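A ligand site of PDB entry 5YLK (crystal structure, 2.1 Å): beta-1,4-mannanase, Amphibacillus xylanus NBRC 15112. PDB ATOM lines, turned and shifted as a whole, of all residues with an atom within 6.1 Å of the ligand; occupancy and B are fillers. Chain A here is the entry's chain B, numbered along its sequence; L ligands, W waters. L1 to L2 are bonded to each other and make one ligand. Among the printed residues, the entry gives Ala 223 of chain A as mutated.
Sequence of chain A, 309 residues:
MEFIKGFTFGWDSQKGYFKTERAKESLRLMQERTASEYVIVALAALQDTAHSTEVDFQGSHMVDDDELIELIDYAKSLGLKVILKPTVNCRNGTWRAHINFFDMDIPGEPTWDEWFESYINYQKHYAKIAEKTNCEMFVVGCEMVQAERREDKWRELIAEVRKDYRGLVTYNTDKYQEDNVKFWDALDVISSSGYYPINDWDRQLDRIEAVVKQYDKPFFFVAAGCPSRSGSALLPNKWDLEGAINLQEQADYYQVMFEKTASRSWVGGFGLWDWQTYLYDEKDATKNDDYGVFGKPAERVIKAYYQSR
The side-chain carboxylate of Glu 143 is in salt-bridge range of the guanidinium group of Arg 96, 2.9 Å away.
OE1 of Glu 143 is in hydrogen-bond range of NE1 of Trp 95, at 3.1 Å.
O of Asn 172 lies within hydrogen-bond range of N of Glu 143.
The backbone carbonyl oxygen (O) of Asn 237 sits at hydrogen-bond distance from the side-chain hydroxyl (OH) of Tyr 291 (3.2 Å).
NH2 of Arg 96 lies within hydrogen-bond range of OD1 of Asn 89.
The guanidinium group (NH1) of Arg 96 is in hydrogen-bond range of the side-chain sulfur (SG) of Cys 142.
The side-chain hydroxyl (OH) of Tyr 291 is in hydrogen-bond range of the backbone carbonyl oxygen (O) of Pro 236 (2.6 Å).
The side-chain hydroxyl (OG) of Ser 193 sits at hydrogen-bond distance from the side-chain amide oxygen (OD1) of Asn 172 (3.1 Å).
Water W2 bridges an oxygen (O6) of LIG L1 and the backbone carbonyl oxygen (O) of Asn 237.
Water W1 bridges OD1 of Asp 290 and O2 of LG2 L2.
OG of Ser 193 touches O1 of LIG L1, 3.7 Å away.
CB of Ala 223 touches O1 of LIG L1 (3.8 Å).
Trp 239 touches the ligand.
Within 4 Å of the ligand: Trp 11, Asn 89, Arg 96, Glu 143, Ser 193, Tyr 195, Ala 223, Asn 237, Trp 239, Trp 273 and Tyr 291.
The nearest printed residue that does not touch the ligand is Trp 95 (4.2 Å).
The side-chain carboxylate (OE2) of Glu 143 lies within hydrogen-bond range of an oxygen (O1) of LIG L1 (2.4 Å).
OH of Tyr 195 is in hydrogen-bond range of O5 of LIG L1 (2.7 Å).
An oxygen (O6) of LIG L1 sits at hydrogen-bond distance from the backbone carbonyl oxygen (O) of Asn 237 (2.8 Å).
The guanidinium group (NH2) of Arg 96 sits at hydrogen-bond distance from an oxygen (O3) of LIG L1 (2.8 Å).
The indole nitrogen (NE1) of Trp 11 lies within hydrogen-bond range of an oxygen (O4) of LG2 L2 (3.1 Å).
OH of Tyr 291 lies within hydrogen-bond range of O6 of LIG L1.
O5 of LG2 L2 sits at hydrogen-bond distance from ND2 of Asn 89, 3.3 Å away.
An oxygen (O4) of LIG L1 is in hydrogen-bond range of the indole nitrogen (NE1) of Trp 273 (3.4 Å).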
ATOM      1  N   TRP A  11      32.177   9.847 -29.348  1.00  0.00           N
ATOM      2  CA  TRP A  11      31.411   8.603 -29.449  1.00  0.00           C
ATOM      3  C   TRP A  11      31.730   7.852 -30.742  1.00  0.00           C
ATOM      4  O   TRP A  11      31.624   6.620 -30.787  1.00  0.00           O
ATOM      5  CB  TRP A  11      29.920   8.903 -29.395  1.00  0.00           C
ATOM      6  CG  TRP A  11      29.016   7.689 -29.256  1.00  0.00           C
ATOM      7  CD1 TRP A  11      27.957   7.371 -30.069  1.00  0.00           C
ATOM      8  CD2 TRP A  11      29.068   6.664 -28.257  1.00  0.00           C
ATOM      9  NE1 TRP A  11      27.353   6.216 -29.635  1.00  0.00           N
ATOM     10  CE2 TRP A  11      28.009   5.767 -28.526  1.00  0.00           C
ATOM     11  CE3 TRP A  11      29.885   6.428 -27.147  1.00  0.00           C
ATOM     12  CZ2 TRP A  11      27.758   4.632 -27.720  1.00  0.00           C
ATOM     13  CZ3 TRP A  11      29.640   5.320 -26.353  1.00  0.00           C
ATOM     14  CH2 TRP A  11      28.582   4.426 -26.639  1.00  0.00           C
ATOM     15  N   LYS A  85      33.517   8.525 -19.510  1.00  0.00           N
ATOM     16  CA  LYS A  85      32.308   7.695 -19.513  1.00  0.00           C
ATOM     17  C   LYS A  85      32.549   6.447 -20.370  1.00  0.00           C
ATOM     18  O   LYS A  85      32.233   6.420 -21.562  1.00  0.00           O
ATOM     19  CB  LYS A  85      31.109   8.489 -20.016  1.00  0.00           C
ATOM     20  CG  LYS A  85      29.824   7.683 -20.105  1.00  0.00           C
ATOM     21  CD  LYS A  85      28.636   8.595 -20.470  1.00  0.00           C
ATOM     22  CE  LYS A  85      27.682   7.892 -21.416  1.00  0.00           C
ATOM     23  NZ  LYS A  85      26.490   8.746 -21.729  1.00  0.00           N
ATOM     24  N   ASN A  89      28.834  -1.591 -25.827  1.00  0.00           N
ATOM     25  CA  ASN A  89      27.853  -1.852 -26.875  1.00  0.00           C
ATOM     26  C   ASN A  89      27.889  -3.324 -27.233  1.00  0.00           C
ATOM     27  O   ASN A  89      28.859  -4.044 -26.943  1.00  0.00           O
ATOM     28  CB  ASN A  89      28.117  -0.987 -28.138  1.00  0.00           C
ATOM     29  CG  ASN A  89      27.841   0.501 -27.910  1.00  0.00           C
ATOM     30  OD1 ASN A  89      27.212   0.894 -26.930  1.00  0.00           O
ATOM     31  ND2 ASN A  89      28.320   1.337 -28.834  1.00  0.00           N
ATOM     32  N   TRP A  95      20.667  -2.757 -27.801  1.00  0.00           N
ATOM     33  CA  TRP A  95      20.854  -1.713 -26.803  1.00  0.00           C
ATOM     34  C   TRP A  95      21.346  -2.321 -25.483  1.00  0.00           C
ATOM     35  O   TRP A  95      20.823  -3.334 -25.005  1.00  0.00           O
ATOM     36  CB  TRP A  95      19.524  -0.983 -26.602  1.00  0.00           C
ATOM     37  CG  TRP A  95      19.556   0.179 -25.670  1.00  0.00           C
ATOM     38  CD1 TRP A  95      20.620   0.976 -25.381  1.00  0.00           C
ATOM     39  CD2 TRP A  95      18.453   0.691 -24.920  1.00  0.00           C
ATOM     40  NE1 TRP A  95      20.259   1.940 -24.486  1.00  0.00           N
ATOM     41  CE2 TRP A  95      18.930   1.792 -24.182  1.00  0.00           C
ATOM     42  CE3 TRP A  95      17.112   0.308 -24.772  1.00  0.00           C
ATOM     43  CZ2 TRP A  95      18.118   2.524 -23.322  1.00  0.00           C
ATOM     44  CZ3 TRP A  95      16.306   1.037 -23.924  1.00  0.00           C
ATOM     45  CH2 TRP A  95      16.818   2.138 -23.209  1.00  0.00           C
ATOM     46  N   ARG A  96      22.373  -1.690 -24.887  1.00  0.00           N
ATOM     47  CA  ARG A  96      23.008  -2.236 -23.698  1.00  0.00           C
ATOM     48  C   ARG A  96      22.043  -2.352 -22.519  1.00  0.00           C
ATOM     49  O   ARG A  96      22.318  -3.111 -21.583  1.00  0.00           O
ATOM     50  CB  ARG A  96      24.209  -1.372 -23.286  1.00  0.00           C
ATOM     51  CG  ARG A  96      23.797  -0.047 -22.647  1.00  0.00           C
ATOM     52  CD  ARG A  96      24.974   0.904 -22.512  1.00  0.00           C
ATOM     53  NE  ARG A  96      25.473   1.363 -23.798  1.00  0.00           N
ATOM     54  CZ  ARG A  96      24.946   2.372 -24.485  1.00  0.00           C
ATOM     55  NH1 ARG A  96      23.910   3.037 -23.986  1.00  0.00           N
ATOM     56  NH2 ARG A  96      25.459   2.722 -25.665  1.00  0.00           N
ATOM     57  N   CYS A 142      26.185   3.058 -17.959  1.00  0.00           N
ATOM     58  CA  CYS A 142      25.278   3.866 -18.767  1.00  0.00           C
ATOM     59  C   CYS A 142      24.059   3.042 -19.141  1.00  0.00           C
ATOM     60  O   CYS A 142      24.180   2.029 -19.850  1.00  0.00           O
ATOM     61  CB  CYS A 142      25.989   4.354 -20.038  1.00  0.00           C
ATOM     62  SG  CYS A 142      24.950   5.321 -21.144  1.00  0.00           S
ATOM     63  N   GLU A 143      22.884   3.474 -18.658  1.00  0.00           N
ATOM     64  CA  GLU A 143      21.598   2.954 -19.111  1.00  0.00           C
ATOM     65  C   GLU A 143      21.508   1.439 -19.003  1.00  0.00           C
ATOM     66  O   GLU A 143      20.909   0.777 -19.857  1.00  0.00           O
ATOM     67  CB  GLU A 143      21.289   3.407 -20.544  1.00  0.00           C
ATOM     68  CG  GLU A 143      21.242   4.910 -20.757  1.00  0.00           C
ATOM     69  CD  GLU A 143      21.286   5.290 -22.240  1.00  0.00           C
ATOM     70  OE1 GLU A 143      21.459   4.389 -23.089  1.00  0.00           O
ATOM     71  OE2 GLU A 143      21.134   6.498 -22.559  1.00  0.00           O
ATOM     72  N   ASN A 172      25.194   6.447 -14.679  1.00  0.00           N
ATOM     73  CA  ASN A 172      24.274   7.071 -15.632  1.00  0.00           C
ATOM     74  C   ASN A 172      23.102   6.124 -15.855  1.00  0.00           C
ATOM     75  O   ASN A 172      23.169   5.199 -16.669  1.00  0.00           O
ATOM     76  CB  ASN A 172      25.021   7.389 -16.938  1.00  0.00           C
ATOM     77  CG  ASN A 172      24.121   7.908 -18.049  1.00  0.00           C
ATOM     78  OD1 ASN A 172      22.922   8.162 -17.863  1.00  0.00           O
ATOM     79  ND2 ASN A 172      24.695   8.095 -19.220  1.00  0.00           N
ATOM     80  N   SER A 193      20.030   9.694 -18.176  1.00  0.00           N
ATOM     81  CA  SER A 193      19.854  10.059 -19.578  1.00  0.00           C
ATOM     82  C   SER A 193      18.503  10.741 -19.682  1.00  0.00           C
ATOM     83  O   SER A 193      17.459  10.077 -19.671  1.00  0.00           O
ATOM     84  CB  SER A 193      19.950   8.846 -20.482  1.00  0.00           C
ATOM     85  OG  SER A 193      21.260   8.310 -20.484  1.00  0.00           O
ATOM     86  N   TYR A 195      16.314  11.898 -21.720  1.00  0.00           N
ATOM     87  CA  TYR A 195      15.591  11.919 -23.004  1.00  0.00           C
ATOM     88  C   TYR A 195      14.082  11.875 -22.734  1.00  0.00           C
ATOM     89  O   TYR A 195      13.401  10.884 -22.986  1.00  0.00           O
ATOM     90  CB  TYR A 195      16.002  10.742 -23.884  1.00  0.00           C
ATOM     91  CG  TYR A 195      17.453  10.711 -24.277  1.00  0.00           C
ATOM     92  CD1 TYR A 195      17.997  11.732 -25.054  1.00  0.00           C
ATOM     93  CD2 TYR A 195      18.273   9.663 -23.888  1.00  0.00           C
ATOM     94  CE1 TYR A 195      19.355  11.708 -25.429  1.00  0.00           C
ATOM     95  CE2 TYR A 195      19.621   9.625 -24.249  1.00  0.00           C
ATOM     96  CZ  TYR A 195      20.145  10.652 -25.013  1.00  0.00           C
ATOM     97  OH  TYR A 195      21.483  10.601 -25.359  1.00  0.00           O
ATOM     98  N   ALA A 223      23.553  12.531 -20.059  1.00  0.00           N
ATOM     99  CA  ALA A 223      23.237  12.508 -21.487  1.00  0.00           C
ATOM    100  C   ALA A 223      21.871  13.144 -21.684  1.00  0.00           C
ATOM    101  O   ALA A 223      20.962  12.973 -20.851  1.00  0.00           O
ATOM    102  CB  ALA A 223      23.256  11.086 -22.077  1.00  0.00           C
ATOM    103  N   PRO A 236      13.215  11.289 -28.010  1.00  0.00           N
ATOM    104  CA  PRO A 236      14.551  11.798 -28.379  1.00  0.00           C
ATOM    105  C   PRO A 236      15.685  10.805 -28.173  1.00  0.00           C
ATOM    106  O   PRO A 236      16.761  10.969 -28.768  1.00  0.00           O
ATOM    107  CB  PRO A 236      14.710  13.038 -27.493  1.00  0.00           C
ATOM    108  CG  PRO A 236      13.854  12.738 -26.286  1.00  0.00           C
ATOM    109  CD  PRO A 236      12.663  11.962 -26.821  1.00  0.00           C
ATOM    110  N   ASN A 237      15.473   9.770 -27.358  1.00  0.00           N
ATOM    111  CA  ASN A 237      16.456   8.701 -27.183  1.00  0.00           C
ATOM    112  C   ASN A 237      16.540   7.783 -28.403  1.00  0.00           C
ATOM    113  O   ASN A 237      17.541   7.073 -28.553  1.00  0.00           O
ATOM    114  CB  ASN A 237      16.061   7.851 -25.995  1.00  0.00           C
ATOM    115  CG  ASN A 237      14.692   7.223 -26.195  1.00  0.00           C
ATOM    116  OD1 ASN A 237      13.694   7.951 -26.307  1.00  0.00           O
ATOM    117  ND2 ASN A 237      14.642   5.909 -26.345  1.00  0.00           N
ATOM    118  N   LYS A 238      15.495   7.735 -29.230  1.00  0.00           N
ATOM    119  CA  LYS A 238      15.422   6.684 -30.251  1.00  0.00           C
ATOM    120  C   LYS A 238      16.299   7.093 -31.411  1.00  0.00           C
ATOM    121  O   LYS A 238      15.882   7.805 -32.324  1.00  0.00           O
ATOM    122  CB  LYS A 238      13.982   6.454 -30.692  1.00  0.00           C
ATOM    123  CG  LYS A 238      13.229   5.410 -29.883  1.00  0.00           C
ATOM    124  CD  LYS A 238      12.035   4.865 -30.664  1.00  0.00           C
ATOM    125  CE  LYS A 238      11.633   3.482 -30.186  1.00  0.00           C
ATOM    126  NZ  LYS A 238      12.671   2.873 -29.316  1.00  0.00           N
ATOM    127  N   TRP A 239      17.560   6.646 -31.371  1.00  0.00           N
ATOM    128  CA  TRP A 239      18.490   7.047 -32.414  1.00  0.00           C
ATOM    129  C   TRP A 239      18.125   6.485 -33.785  1.00  0.00           C
ATOM    130  O   TRP A 239      18.521   7.054 -34.802  1.00  0.00           O
ATOM    131  CB  TRP A 239      19.918   6.637 -32.026  1.00  0.00           C
ATOM    132  CG  TRP A 239      20.126   5.167 -31.814  1.00  0.00           C
ATOM    133  CD1 TRP A 239      20.140   4.495 -30.617  1.00  0.00           C
ATOM    134  CD2 TRP A 239      20.398   4.185 -32.821  1.00  0.00           C
ATOM    135  NE1 TRP A 239      20.389   3.161 -30.824  1.00  0.00           N
ATOM    136  CE2 TRP A 239      20.552   2.938 -32.167  1.00  0.00           C
ATOM    137  CE3 TRP A 239      20.516   4.229 -34.214  1.00  0.00           C
ATOM    138  CZ2 TRP A 239      20.816   1.761 -32.861  1.00  0.00           C
ATOM    139  CZ3 TRP A 239      20.782   3.059 -34.900  1.00  0.00           C
ATOM    140  CH2 TRP A 239      20.929   1.841 -34.217  1.00  0.00           C
ATOM    141  N   TRP A 273      24.229  15.226 -26.092  1.00  0.00           N
ATOM    142  CA  TRP A 273      24.577  14.123 -26.981  1.00  0.00           C
ATOM    143  C   TRP A 273      24.241  14.522 -28.414  1.00  0.00           C
ATOM    144  O   TRP A 273      23.076  14.803 -28.712  1.00  0.00           O
ATOM    145  CB  TRP A 273      23.800  12.858 -26.597  1.00  0.00           C
ATOM    146  CG  TRP A 273      24.359  11.630 -27.237  1.00  0.00           C
ATOM    147  CD1 TRP A 273      24.162  11.207 -28.528  1.00  0.00           C
ATOM    148  CD2 TRP A 273      25.243  10.692 -26.634  1.00  0.00           C
ATOM    149  NE1 TRP A 273      24.877  10.052 -28.754  1.00  0.00           N
ATOM    150  CE2 TRP A 273      25.546   9.713 -27.610  1.00  0.00           C
ATOM    151  CE3 TRP A 273      25.818  10.578 -25.367  1.00  0.00           C
ATOM    152  CZ2 TRP A 273      26.397   8.633 -27.351  1.00  0.00           C
ATOM    153  CZ3 TRP A 273      26.664   9.505 -25.113  1.00  0.00           C
ATOM    154  CH2 TRP A 273      26.938   8.556 -26.094  1.00  0.00           C
ATOM    155  N   ASP A 274      25.238  14.580 -29.304  1.00  0.00           N
ATOM    156  CA  ASP A 274      26.678  14.389 -29.046  1.00  0.00           C
ATOM    157  C   ASP A 274      27.471  15.154 -30.121  1.00  0.00           C
ATOM    158  O   ASP A 274      26.909  15.531 -31.149  1.00  0.00           O
ATOM    159  CB  ASP A 274      27.073  12.912 -29.081  1.00  0.00           C
ATOM    160  CG  ASP A 274      27.077  12.317 -30.488  1.00  0.00           C
ATOM    161  OD1 ASP A 274      26.078  12.471 -31.206  1.00  0.00           O
ATOM    162  OD2 ASP A 274      28.097  11.687 -30.892  1.00  0.00           O
ATOM    163  N   ASP A 290      21.023  13.698 -37.579  1.00  0.00           N
ATOM    164  CA  ASP A 290      21.666  13.019 -36.466  1.00  0.00           C
ATOM    165  C   ASP A 290      21.576  13.907 -35.217  1.00  0.00           C
ATOM    166  O   ASP A 290      21.006  15.002 -35.219  1.00  0.00           O
ATOM    167  CB  ASP A 290      23.116  12.715 -36.846  1.00  0.00           C
ATOM    168  CG  ASP A 290      23.814  11.748 -35.899  1.00  0.00           C
ATOM    169  OD1 ASP A 290      23.159  11.153 -35.010  1.00  0.00           O
ATOM    170  OD2 ASP A 290      25.048  11.604 -36.054  1.00  0.00           O
ATOM    171  N   TYR A 291      22.163  13.418 -34.123  1.00  0.00           N
ATOM    172  CA  TYR A 291      22.138  14.159 -32.868  1.00  0.00           C
ATOM    173  C   TYR A 291      22.926  15.448 -32.923  1.00  0.00           C
ATOM    174  O   TYR A 291      22.657  16.357 -32.138  1.00  0.00           O
ATOM    175  CB  TYR A 291      22.671  13.294 -31.737  1.00  0.00           C
ATOM    176  CG  TYR A 291      21.643  12.328 -31.229  1.00  0.00           C
ATOM    177  CD1 TYR A 291      20.804  12.684 -30.189  1.00  0.00           C
ATOM    178  CD2 TYR A 291      21.505  11.067 -31.800  1.00  0.00           C
ATOM    179  CE1 TYR A 291      19.858  11.819 -29.723  1.00  0.00           C
ATOM    180  CE2 TYR A 291      20.531  10.179 -31.334  1.00  0.00           C
ATOM    181  CZ  TYR A 291      19.715  10.572 -30.292  1.00  0.00           C
ATOM    182  OH  TYR A 291      18.749   9.740 -29.795  1.00  0.00           O
HETATM  183  C1  LIG L   1      23.182   7.660 -25.137  1.00  0.00           C
HETATM  184  C2  LIG L   1      23.549   6.231 -25.481  1.00  0.00           C
HETATM  185  C3  LIG L   1      23.960   6.112 -26.898  1.00  0.00           C
HETATM  186  C4  LIG L   1      22.941   6.662 -27.856  1.00  0.00           C
HETATM  187  C5  LIG L   1      22.476   8.071 -27.442  1.00  0.00           C
HETATM  188  C6  LIG L   1      21.270   8.456 -28.233  1.00  0.00           C
HETATM  189  O1  LIG L   1      22.735   7.745 -23.858  1.00  0.00           O
HETATM  190  O2  LIG L   1      22.374   5.424 -25.296  1.00  0.00           O
HETATM  191  O3  LIG L   1      24.109   4.706 -27.193  1.00  0.00           O
HETATM  192  O4  LIG L   1      23.522   6.981 -28.929  1.00  0.00           O
HETATM  193  O5  LIG L   1      22.069   8.087 -26.029  1.00  0.00           O
HETATM  194  O6  LIG L   1      20.239   7.541 -27.973  1.00  0.00           O
HETATM  195  C1  LG2 L   2      23.478   6.058 -30.017  1.00  0.00           C
HETATM  196  C2  LG2 L   2      23.688   6.798 -31.332  1.00  0.00           C
HETATM  197  C3  LG2 L   2      23.692   5.816 -32.502  1.00  0.00           C
HETATM  198  C4  LG2 L   2      24.667   4.672 -32.231  1.00  0.00           C
HETATM  199  C5  LG2 L   2      24.425   4.062 -30.860  1.00  0.00           C
HETATM  200  C6  LG2 L   2      25.459   2.974 -30.558  1.00  0.00           C
HETATM  201  O1  LG2 L   2      24.933   7.504 -31.295  1.00  0.00           O
HETATM  202  O2  LG2 L   2      24.090   6.503 -33.695  1.00  0.00           O
HETATM  203  O3  LG2 L   2      24.496   3.665 -33.239  1.00  0.00           O
HETATM  204  O4  LG2 L   2      24.512   5.083 -29.857  1.00  0.00           O
HETATM  205  O5  LG2 L   2      25.273   2.507 -29.220  1.00  0.00           O
HETATM  206  O   HOH W   1      22.439   8.699 -34.027  1.00  0.00           O
HETATM  207  O   HOH W   2      19.499   6.148 -25.969  1.00  0.00           O
